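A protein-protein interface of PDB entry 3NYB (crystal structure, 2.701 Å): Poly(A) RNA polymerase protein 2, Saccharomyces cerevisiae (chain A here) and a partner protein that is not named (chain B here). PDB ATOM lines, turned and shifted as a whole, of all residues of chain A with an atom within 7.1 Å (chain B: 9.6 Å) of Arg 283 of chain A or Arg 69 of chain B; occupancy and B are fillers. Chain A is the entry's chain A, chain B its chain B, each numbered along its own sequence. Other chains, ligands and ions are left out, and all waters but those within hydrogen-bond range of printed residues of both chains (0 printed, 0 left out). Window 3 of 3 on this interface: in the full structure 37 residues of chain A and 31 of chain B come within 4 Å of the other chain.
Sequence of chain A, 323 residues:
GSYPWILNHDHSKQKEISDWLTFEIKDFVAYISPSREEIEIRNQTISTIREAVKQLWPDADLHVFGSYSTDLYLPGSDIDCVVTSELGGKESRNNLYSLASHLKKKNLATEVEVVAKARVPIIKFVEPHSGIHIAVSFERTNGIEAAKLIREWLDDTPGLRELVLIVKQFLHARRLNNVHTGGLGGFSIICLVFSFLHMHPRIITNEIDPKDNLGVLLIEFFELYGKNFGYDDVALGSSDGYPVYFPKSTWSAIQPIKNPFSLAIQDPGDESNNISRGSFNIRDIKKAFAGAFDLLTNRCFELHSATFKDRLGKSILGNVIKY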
ATOM      1  N   GLY A 182       0.759 -16.093  26.185  1.00  0.00           N
ATOM      2  CA  GLY A 182      -0.565 -15.575  25.879  1.00  0.00           C
ATOM      3  C   GLY A 182      -0.740 -14.073  26.012  1.00  0.00           C
ATOM      4  O   GLY A 182      -1.865 -13.599  26.149  1.00  0.00           O
ATOM      5  N   LYS A 227     -12.689  -1.584  29.303  1.00  0.00           N
ATOM      6  CA  LYS A 227     -14.031  -1.557  29.883  1.00  0.00           C
ATOM      7  C   LYS A 227     -15.176  -1.782  28.904  1.00  0.00           C
ATOM      8  O   LYS A 227     -16.238  -2.247  29.304  1.00  0.00           O
ATOM      9  CB  LYS A 227     -14.254  -0.241  30.627  1.00  0.00           C
ATOM     10  CG  LYS A 227     -13.412  -0.107  31.896  1.00  0.00           C
ATOM     11  CD  LYS A 227     -13.361   1.329  32.403  1.00  0.00           C
ATOM     12  CE  LYS A 227     -14.716   1.823  32.899  1.00  0.00           C
ATOM     13  NZ  LYS A 227     -14.735   3.311  33.079  1.00  0.00           N
ATOM     14  N   ASP A 232     -15.902 -10.402  22.746  1.00  0.00           N
ATOM     15  CA  ASP A 232     -16.673 -11.562  22.317  1.00  0.00           C
ATOM     16  C   ASP A 232     -17.159 -11.428  20.877  1.00  0.00           C
ATOM     17  O   ASP A 232     -17.079 -12.383  20.108  1.00  0.00           O
ATOM     18  CB  ASP A 232     -17.868 -11.792  23.254  1.00  0.00           C
ATOM     19  CG  ASP A 232     -17.474 -12.478  24.553  1.00  0.00           C
ATOM     20  OD1 ASP A 232     -17.182 -13.695  24.527  1.00  0.00           O
ATOM     21  OD2 ASP A 232     -17.470 -11.801  25.602  1.00  0.00           O
ATOM     22  N   ASN A 259     -13.113 -20.978  21.001  1.00  0.00           N
ATOM     23  CA  ASN A 259     -13.052 -20.078  22.152  1.00  0.00           C
ATOM     24  C   ASN A 259     -13.526 -18.669  21.813  1.00  0.00           C
ATOM     25  O   ASN A 259     -12.803 -17.902  21.178  1.00  0.00           O
ATOM     26  CB  ASN A 259     -11.634 -20.035  22.729  1.00  0.00           C
ATOM     27  CG  ASN A 259     -11.480 -19.003  23.834  1.00  0.00           C
ATOM     28  OD1 ASN A 259     -12.466 -18.514  24.389  1.00  0.00           O
ATOM     29  ND2 ASN A 259     -10.235 -18.669  24.159  1.00  0.00           N
ATOM     30  N   PRO A 260     -14.748 -18.325  22.246  1.00  0.00           N
ATOM     31  CA  PRO A 260     -15.409 -17.041  21.972  1.00  0.00           C
ATOM     32  C   PRO A 260     -14.636 -15.815  22.476  1.00  0.00           C
ATOM     33  O   PRO A 260     -14.450 -14.863  21.717  1.00  0.00           O
ATOM     34  CB  PRO A 260     -16.739 -17.173  22.733  1.00  0.00           C
ATOM     35  CG  PRO A 260     -16.487 -18.269  23.740  1.00  0.00           C
ATOM     36  CD  PRO A 260     -15.642 -19.231  22.982  1.00  0.00           C
ATOM     37  N   PHE A 261     -14.202 -15.841  23.733  1.00  0.00           N
ATOM     38  CA  PHE A 261     -13.574 -14.672  24.347  1.00  0.00           C
ATOM     39  C   PHE A 261     -12.083 -14.565  24.042  1.00  0.00           C
ATOM     40  O   PHE A 261     -11.244 -15.105  24.764  1.00  0.00           O
ATOM     41  CB  PHE A 261     -13.798 -14.670  25.859  1.00  0.00           C
ATOM     42  CG  PHE A 261     -13.388 -13.387  26.528  1.00  0.00           C
ATOM     43  CD1 PHE A 261     -14.204 -12.273  26.472  1.00  0.00           C
ATOM     44  CD2 PHE A 261     -12.197 -13.299  27.218  1.00  0.00           C
ATOM     45  CE1 PHE A 261     -13.837 -11.093  27.086  1.00  0.00           C
ATOM     46  CE2 PHE A 261     -11.823 -12.121  27.837  1.00  0.00           C
ATOM     47  CZ  PHE A 261     -12.646 -11.016  27.769  1.00  0.00           C
ATOM     48  N   SER A 262     -11.761 -13.847  22.976  1.00  0.00           N
ATOM     49  CA  SER A 262     -10.380 -13.705  22.549  1.00  0.00           C
ATOM     50  C   SER A 262     -10.246 -12.603  21.500  1.00  0.00           C
ATOM     51  O   SER A 262     -11.174 -12.340  20.736  1.00  0.00           O
ATOM     52  CB  SER A 262      -9.852 -15.036  22.004  1.00  0.00           C
ATOM     53  OG  SER A 262     -10.585 -15.450  20.866  1.00  0.00           O
ATOM     54  N   SER A 279      -2.959 -14.964  21.626  1.00  0.00           N
ATOM     55  CA  SER A 279      -3.085 -14.229  22.879  1.00  0.00           C
ATOM     56  C   SER A 279      -4.184 -14.810  23.767  1.00  0.00           C
ATOM     57  O   SER A 279      -5.234 -14.204  23.950  1.00  0.00           O
ATOM     58  CB  SER A 279      -3.348 -12.750  22.604  1.00  0.00           C
ATOM     59  OG  SER A 279      -2.263 -12.171  21.902  1.00  0.00           O
ATOM     60  N   PHE A 280      -3.936 -15.986  24.328  1.00  0.00           N
ATOM     61  CA  PHE A 280      -4.975 -16.686  25.070  1.00  0.00           C
ATOM     62  C   PHE A 280      -5.236 -16.081  26.450  1.00  0.00           C
ATOM     63  O   PHE A 280      -6.235 -16.395  27.103  1.00  0.00           O
ATOM     64  CB  PHE A 280      -4.668 -18.183  25.173  1.00  0.00           C
ATOM     65  CG  PHE A 280      -3.274 -18.503  25.662  1.00  0.00           C
ATOM     66  CD1 PHE A 280      -2.991 -18.539  27.018  1.00  0.00           C
ATOM     67  CD2 PHE A 280      -2.255 -18.804  24.762  1.00  0.00           C
ATOM     68  CE1 PHE A 280      -1.717 -18.848  27.472  1.00  0.00           C
ATOM     69  CE2 PHE A 280      -0.973 -19.119  25.208  1.00  0.00           C
ATOM     70  CZ  PHE A 280      -0.707 -19.140  26.566  1.00  0.00           C
ATOM     71  N   ASN A 281      -4.347 -15.203  26.890  1.00  0.00           N
ATOM     72  CA  ASN A 281      -4.495 -14.627  28.213  1.00  0.00           C
ATOM     73  C   ASN A 281      -5.239 -13.315  28.154  1.00  0.00           C
ATOM     74  O   ASN A 281      -5.065 -12.440  28.997  1.00  0.00           O
ATOM     75  CB  ASN A 281      -3.144 -14.437  28.878  1.00  0.00           C
ATOM     76  CG  ASN A 281      -3.248 -14.414  30.383  1.00  0.00           C
ATOM     77  OD1 ASN A 281      -2.363 -13.905  31.063  1.00  0.00           O
ATOM     78  ND2 ASN A 281      -4.339 -14.967  30.912  1.00  0.00           N
ATOM     79  N   ILE A 282      -6.083 -13.195  27.144  1.00  0.00           N
ATOM     80  CA  ILE A 282      -6.771 -11.955  26.866  1.00  0.00           C
ATOM     81  C   ILE A 282      -7.647 -11.512  28.034  1.00  0.00           C
ATOM     82  O   ILE A 282      -7.887 -10.327  28.221  1.00  0.00           O
ATOM     83  CB  ILE A 282      -7.601 -12.093  25.580  1.00  0.00           C
ATOM     84  CG1 ILE A 282      -8.347 -10.793  25.280  1.00  0.00           C
ATOM     85  CG2 ILE A 282      -8.525 -13.310  25.664  1.00  0.00           C
ATOM     86  CD1 ILE A 282      -7.446  -9.706  24.776  1.00  0.00           C
ATOM     87  N   ARG A 283      -8.116 -12.461  28.831  1.00  0.00           N
ATOM     88  CA  ARG A 283      -8.951 -12.119  29.977  1.00  0.00           C
ATOM     89  C   ARG A 283      -8.216 -11.221  30.965  1.00  0.00           C
ATOM     90  O   ARG A 283      -8.756 -10.216  31.421  1.00  0.00           O
ATOM     91  CB  ARG A 283      -9.418 -13.382  30.688  1.00  0.00           C
ATOM     92  CG  ARG A 283     -10.031 -14.402  29.764  1.00  0.00           C
ATOM     93  CD  ARG A 283     -10.693 -15.509  30.556  1.00  0.00           C
ATOM     94  NE  ARG A 283     -11.435 -16.419  29.691  1.00  0.00           N
ATOM     95  CZ  ARG A 283     -12.690 -16.222  29.306  1.00  0.00           C
ATOM     96  NH1 ARG A 283     -13.345 -15.143  29.715  1.00  0.00           N
ATOM     97  NH2 ARG A 283     -13.290 -17.100  28.514  1.00  0.00           N
ATOM     98  N   ASP A 284      -6.990 -11.603  31.306  1.00  0.00           N
ATOM     99  CA  ASP A 284      -6.169 -10.830  32.233  1.00  0.00           C
ATOM    100  C   ASP A 284      -5.665  -9.548  31.592  1.00  0.00           C
ATOM    101  O   ASP A 284      -5.400  -8.561  32.275  1.00  0.00           O
ATOM    102  CB  ASP A 284      -4.988 -11.662  32.727  1.00  0.00           C
ATOM    103  CG  ASP A 284      -5.385 -12.641  33.814  1.00  0.00           C
ATOM    104  OD1 ASP A 284      -6.599 -12.881  33.980  1.00  0.00           O
ATOM    105  OD2 ASP A 284      -4.488 -13.165  34.509  1.00  0.00           O
ATOM    106  N   ILE A 285      -5.525  -9.565  30.274  1.00  0.00           N
ATOM    107  CA  ILE A 285      -5.102  -8.371  29.561  1.00  0.00           C
ATOM    108  C   ILE A 285      -6.135  -7.265  29.754  1.00  0.00           C
ATOM    109  O   ILE A 285      -5.791  -6.140  30.108  1.00  0.00           O
ATOM    110  CB  ILE A 285      -4.873  -8.663  28.065  1.00  0.00           C
ATOM    111  CG1 ILE A 285      -3.695  -9.626  27.901  1.00  0.00           C
ATOM    112  CG2 ILE A 285      -4.628  -7.372  27.298  1.00  0.00           C
ATOM    113  CD1 ILE A 285      -3.570 -10.219  26.526  1.00  0.00           C
ATOM    114  N   LYS A 286      -7.407  -7.602  29.546  1.00  0.00           N
ATOM    115  CA  LYS A 286      -8.500  -6.653  29.740  1.00  0.00           C
ATOM    116  C   LYS A 286      -8.565  -6.159  31.177  1.00  0.00           C
ATOM    117  O   LYS A 286      -8.766  -4.968  31.421  1.00  0.00           O
ATOM    118  CB  LYS A 286      -9.838  -7.279  29.353  1.00  0.00           C
ATOM    119  CG  LYS A 286     -11.040  -6.398  29.655  1.00  0.00           C
ATOM    120  CD  LYS A 286     -12.323  -7.020  29.134  1.00  0.00           C
ATOM    121  CE  LYS A 286     -13.534  -6.126  29.403  1.00  0.00           C
ATOM    122  NZ  LYS A 286     -14.806  -6.804  29.034  1.00  0.00           N
ATOM    123  N   LYS A 287      -8.404  -7.071  32.130  1.00  0.00           N
ATOM    124  CA  LYS A 287      -8.329  -6.675  33.537  1.00  0.00           C
ATOM    125  C   LYS A 287      -7.231  -5.638  33.762  1.00  0.00           C
ATOM    126  O   LYS A 287      -7.426  -4.674  34.489  1.00  0.00           O
ATOM    127  CB  LYS A 287      -8.107  -7.882  34.459  1.00  0.00           C
ATOM    128  CG  LYS A 287      -9.369  -8.370  35.145  1.00  0.00           C
ATOM    129  CD  LYS A 287      -9.805  -9.745  34.669  1.00  0.00           C
ATOM    130  CE  LYS A 287      -9.071 -10.839  35.439  1.00  0.00           C
ATOM    131  NZ  LYS A 287      -9.807 -12.139  35.440  1.00  0.00           N
ATOM    132  N   ALA A 288      -6.083  -5.833  33.120  1.00  0.00           N
ATOM    133  CA  ALA A 288      -4.940  -4.951  33.320  1.00  0.00           C
ATOM    134  C   ALA A 288      -5.156  -3.547  32.743  1.00  0.00           C
ATOM    135  O   ALA A 288      -4.858  -2.555  33.411  1.00  0.00           O
ATOM    136  CB  ALA A 288      -3.668  -5.582  32.774  1.00  0.00           C
ATOM    137  N   ASN B  51     -19.375  -2.358  20.426  1.00  0.00           N
ATOM    138  CA  ASN B  51     -20.270  -3.322  21.057  1.00  0.00           C
ATOM    139  C   ASN B  51     -20.734  -4.400  20.086  1.00  0.00           C
ATOM    140  O   ASN B  51     -20.694  -5.588  20.394  1.00  0.00           O
ATOM    141  CB  ASN B  51     -21.474  -2.600  21.650  1.00  0.00           C
ATOM    142  CG  ASN B  51     -22.330  -3.506  22.491  1.00  0.00           C
ATOM    143  OD1 ASN B  51     -23.557  -3.437  22.446  1.00  0.00           O
ATOM    144  ND2 ASN B  51     -21.689  -4.375  23.257  1.00  0.00           N
ATOM    145  N   LYS B  65     -27.641  -5.726  23.510  1.00  0.00           N
ATOM    146  CA  LYS B  65     -27.127  -6.023  24.841  1.00  0.00           C
ATOM    147  C   LYS B  65     -25.617  -5.856  24.778  1.00  0.00           C
ATOM    148  O   LYS B  65     -24.988  -6.264  23.801  1.00  0.00           O
ATOM    149  CB  LYS B  65     -27.467  -7.456  25.264  1.00  0.00           C
ATOM    150  CG  LYS B  65     -28.906  -7.677  25.689  1.00  0.00           C
ATOM    151  CD  LYS B  65     -29.029  -8.942  26.526  1.00  0.00           C
ATOM    152  CE  LYS B  65     -30.483  -9.329  26.749  1.00  0.00           C
ATOM    153  NZ  LYS B  65     -31.137  -9.800  25.495  1.00  0.00           N
ATOM    154  N   ARG B  66     -25.030  -5.259  25.810  1.00  0.00           N
ATOM    155  CA  ARG B  66     -23.606  -4.952  25.761  1.00  0.00           C
ATOM    156  C   ARG B  66     -22.713  -6.196  25.888  1.00  0.00           C
ATOM    157  O   ARG B  66     -23.001  -7.111  26.662  1.00  0.00           O
ATOM    158  CB  ARG B  66     -23.234  -3.849  26.763  1.00  0.00           C
ATOM    159  CG  ARG B  66     -22.926  -4.301  28.176  1.00  0.00           C
ATOM    160  CD  ARG B  66     -22.083  -3.236  28.870  1.00  0.00           C
ATOM    161  NE  ARG B  66     -21.216  -2.561  27.903  1.00  0.00           N
ATOM    162  CZ  ARG B  66     -20.276  -1.675  28.215  1.00  0.00           C
ATOM    163  NH1 ARG B  66     -20.057  -1.340  29.478  1.00  0.00           N
ATOM    164  NH2 ARG B  66     -19.551  -1.120  27.256  1.00  0.00           N
ATOM    165  N   SER B  67     -21.637  -6.215  25.104  1.00  0.00           N
ATOM    166  CA  SER B  67     -20.751  -7.371  24.994  1.00  0.00           C
ATOM    167  C   SER B  67     -19.704  -7.439  26.103  1.00  0.00           C
ATOM    168  O   SER B  67     -18.904  -8.370  26.164  1.00  0.00           O
ATOM    169  CB  SER B  67     -20.048  -7.361  23.635  1.00  0.00           C
ATOM    170  OG  SER B  67     -19.014  -8.329  23.585  1.00  0.00           O
ATOM    171  N   SER B  68     -19.707  -6.439  26.970  1.00  0.00           N
ATOM    172  CA  SER B  68     -18.757  -6.392  28.064  1.00  0.00           C
ATOM    173  C   SER B  68     -19.492  -6.443  29.387  1.00  0.00           C
ATOM    174  O   SER B  68     -20.197  -5.505  29.753  1.00  0.00           O
ATOM    175  CB  SER B  68     -17.916  -5.122  27.989  1.00  0.00           C
ATOM    176  OG  SER B  68     -17.110  -4.990  29.144  1.00  0.00           O
ATOM    177  N   ARG B  69     -19.318  -7.545  30.104  1.00  0.00           N
ATOM    178  CA  ARG B  69     -19.945  -7.723  31.404  1.00  0.00           C
ATOM    179  C   ARG B  69     -19.517  -6.638  32.386  1.00  0.00           C
ATOM    180  O   ARG B  69     -19.973  -6.602  33.525  1.00  0.00           O
ATOM    181  CB  ARG B  69     -19.618  -9.111  31.947  1.00  0.00           C
ATOM    182  CG  ARG B  69     -18.341  -9.699  31.376  1.00  0.00           C
ATOM    183  CD  ARG B  69     -18.244 -11.180  31.682  1.00  0.00           C
ATOM    184  NE  ARG B  69     -16.972 -11.742  31.245  1.00  0.00           N
ATOM    185  CZ  ARG B  69     -16.514 -12.928  31.631  1.00  0.00           C
ATOM    186  NH1 ARG B  69     -17.226 -13.675  32.464  1.00  0.00           N
ATOM    187  NH2 ARG B  69     -15.343 -13.365  31.187  1.00  0.00           N
ATOM    188  N   VAL B  70     -18.644  -5.749  31.926  1.00  0.00           N
ATOM    189  CA  VAL B  70     -18.154  -4.640  32.734  1.00  0.00           C
ATOM    190  C   VAL B  70     -19.007  -3.403  32.499  1.00  0.00           C
ATOM    191  O   VAL B  70     -19.251  -3.028  31.358  1.00  0.00           O
ATOM    192  CB  VAL B  70     -16.699  -4.301  32.374  1.00  0.00           C
ATOM    193  CG1 VAL B  70     -16.186  -3.177  33.256  1.00  0.00           C
ATOM    194  CG2 VAL B  70     -15.819  -5.544  32.486  1.00  0.00           C
ATOM    195  N   PRO B  71     -19.461  -2.762  33.584  1.00  0.00           N
ATOM    196  CA  PRO B  71     -20.366  -1.606  33.520  1.00  0.00           C
ATOM    197  C   PRO B  71     -19.692  -0.292  33.127  1.00  0.00           C
ATOM    198  O   PRO B  71     -18.466  -0.190  33.110  1.00  0.00           O
ATOM    199  CB  PRO B  71     -20.889  -1.489  34.960  1.00  0.00           C
ATOM    200  CG  PRO B  71     -20.500  -2.765  35.643  1.00  0.00           C
ATOM    201  CD  PRO B  71     -19.249  -3.208  34.968  1.00  0.00           C
ATOM    202  N   ASN B  72     -20.515   0.700  32.805  1.00  0.00           N
ATOM    203  CA  ASN B  72     -20.076   2.086  32.686  1.00  0.00           C
ATOM    204  C   ASN B  72     -21.271   3.040  32.644  1.00  0.00           C
ATOM    205  O   ASN B  72     -21.523   3.703  31.638  1.00  0.00           O
ATOM    206  CB  ASN B  72     -19.125   2.292  31.491  1.00  0.00           C
ATOM    207  CG  ASN B  72     -19.855   2.432  30.163  1.00  0.00           C
ATOM    208  OD1 ASN B  72     -20.938   1.882  29.974  1.00  0.00           O
ATOM    209  ND2 ASN B  72     -19.257   3.173  29.236  1.00  0.00           N
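The backbone carbonyl oxygen of Lys 227 of chain A sits at hydrogen-bond distance from the side-chain hydroxyl of Ser 68 of chain B (2.9 Å).
OG of Ser 68 of chain B is in hydrogen-bond range of NZ of Lys 286 of chain A (2.9 Å).
NH1 of Arg 283 of chain A sits close to NH2 of Arg 69 of chain B, 3.1 Å away.
The backbone NH of Ser 67 of chain B sits close to the side-chain amide nitrogen of Asn 51 of chain B (2.6 Å).
NH1 of Arg 66 of chain B is in hydrogen-bond range of O of Val 70 of chain B, 2.7 Å away.
NH1 of Arg 66 of chain B lies within hydrogen-bond range of OD1 of Asn 72 of chain B, 3.4 Å away.
N of Val 70 of chain B lies close to OG of Ser 68 of chain B (3.3 Å).
Among the printed residues, merely in contact across the chains: Lys 227 of chain A with Arg 66 of chain B (3.9 Å), Lys 227 of chain A with Val 70 of chain B (3.7 Å), Asp 232 of chain A with Ser 67 of chain B (3.7 Å) and Lys 286 of chain A with Val 70 of chain B (3.8 Å).
Printed residues of chain B within 4 Å of Arg 283 of chain A: Arg 69 (3.1 Å).
Of chain A, only Arg 283 (3.1 Å) comes within 4 Å of Arg 69 of chain B.
Phe 261 of chain A touches none of the printed residues of chain B.
Ile 282 of chain A touches none of the printed residues of chain B.
Printed residues of chain B within 4 Å of Lys 286 of chain A: Ser 68 and Val 70.
Of the printed residues of chain A, Ser 67 of chain B touches Asp 232.
Of the printed residues of chain A, Ser 68 of chain B touches Lys 227 and Lys 286.
Of the printed residues of chain B, Asp 232 of chain A touches Ser 67.
Printed residues of chain B within 4 Å of Lys 227 of chain A: Arg 66 (3.9 Å), Ser 68 (2.9 Å) and Val 70 (3.7 Å).
Lys 287 of chain A touches none of the printed residues of chain B.
Phe 280 of chain A touches none of the printed residues of chain B.
Along chain A the printed residues that touch a printed residue of chain B span positions 227 to 286.
Of the 9 printed residues of chain B, 5 touch a printed residue of chain A.
Hydrophobic or aromatic side chains of chain B within 4 Å of the printed part of chain A: Val 70.
Along chain B the printed residues that touch a printed residue of chain A span positions 66 to 70.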
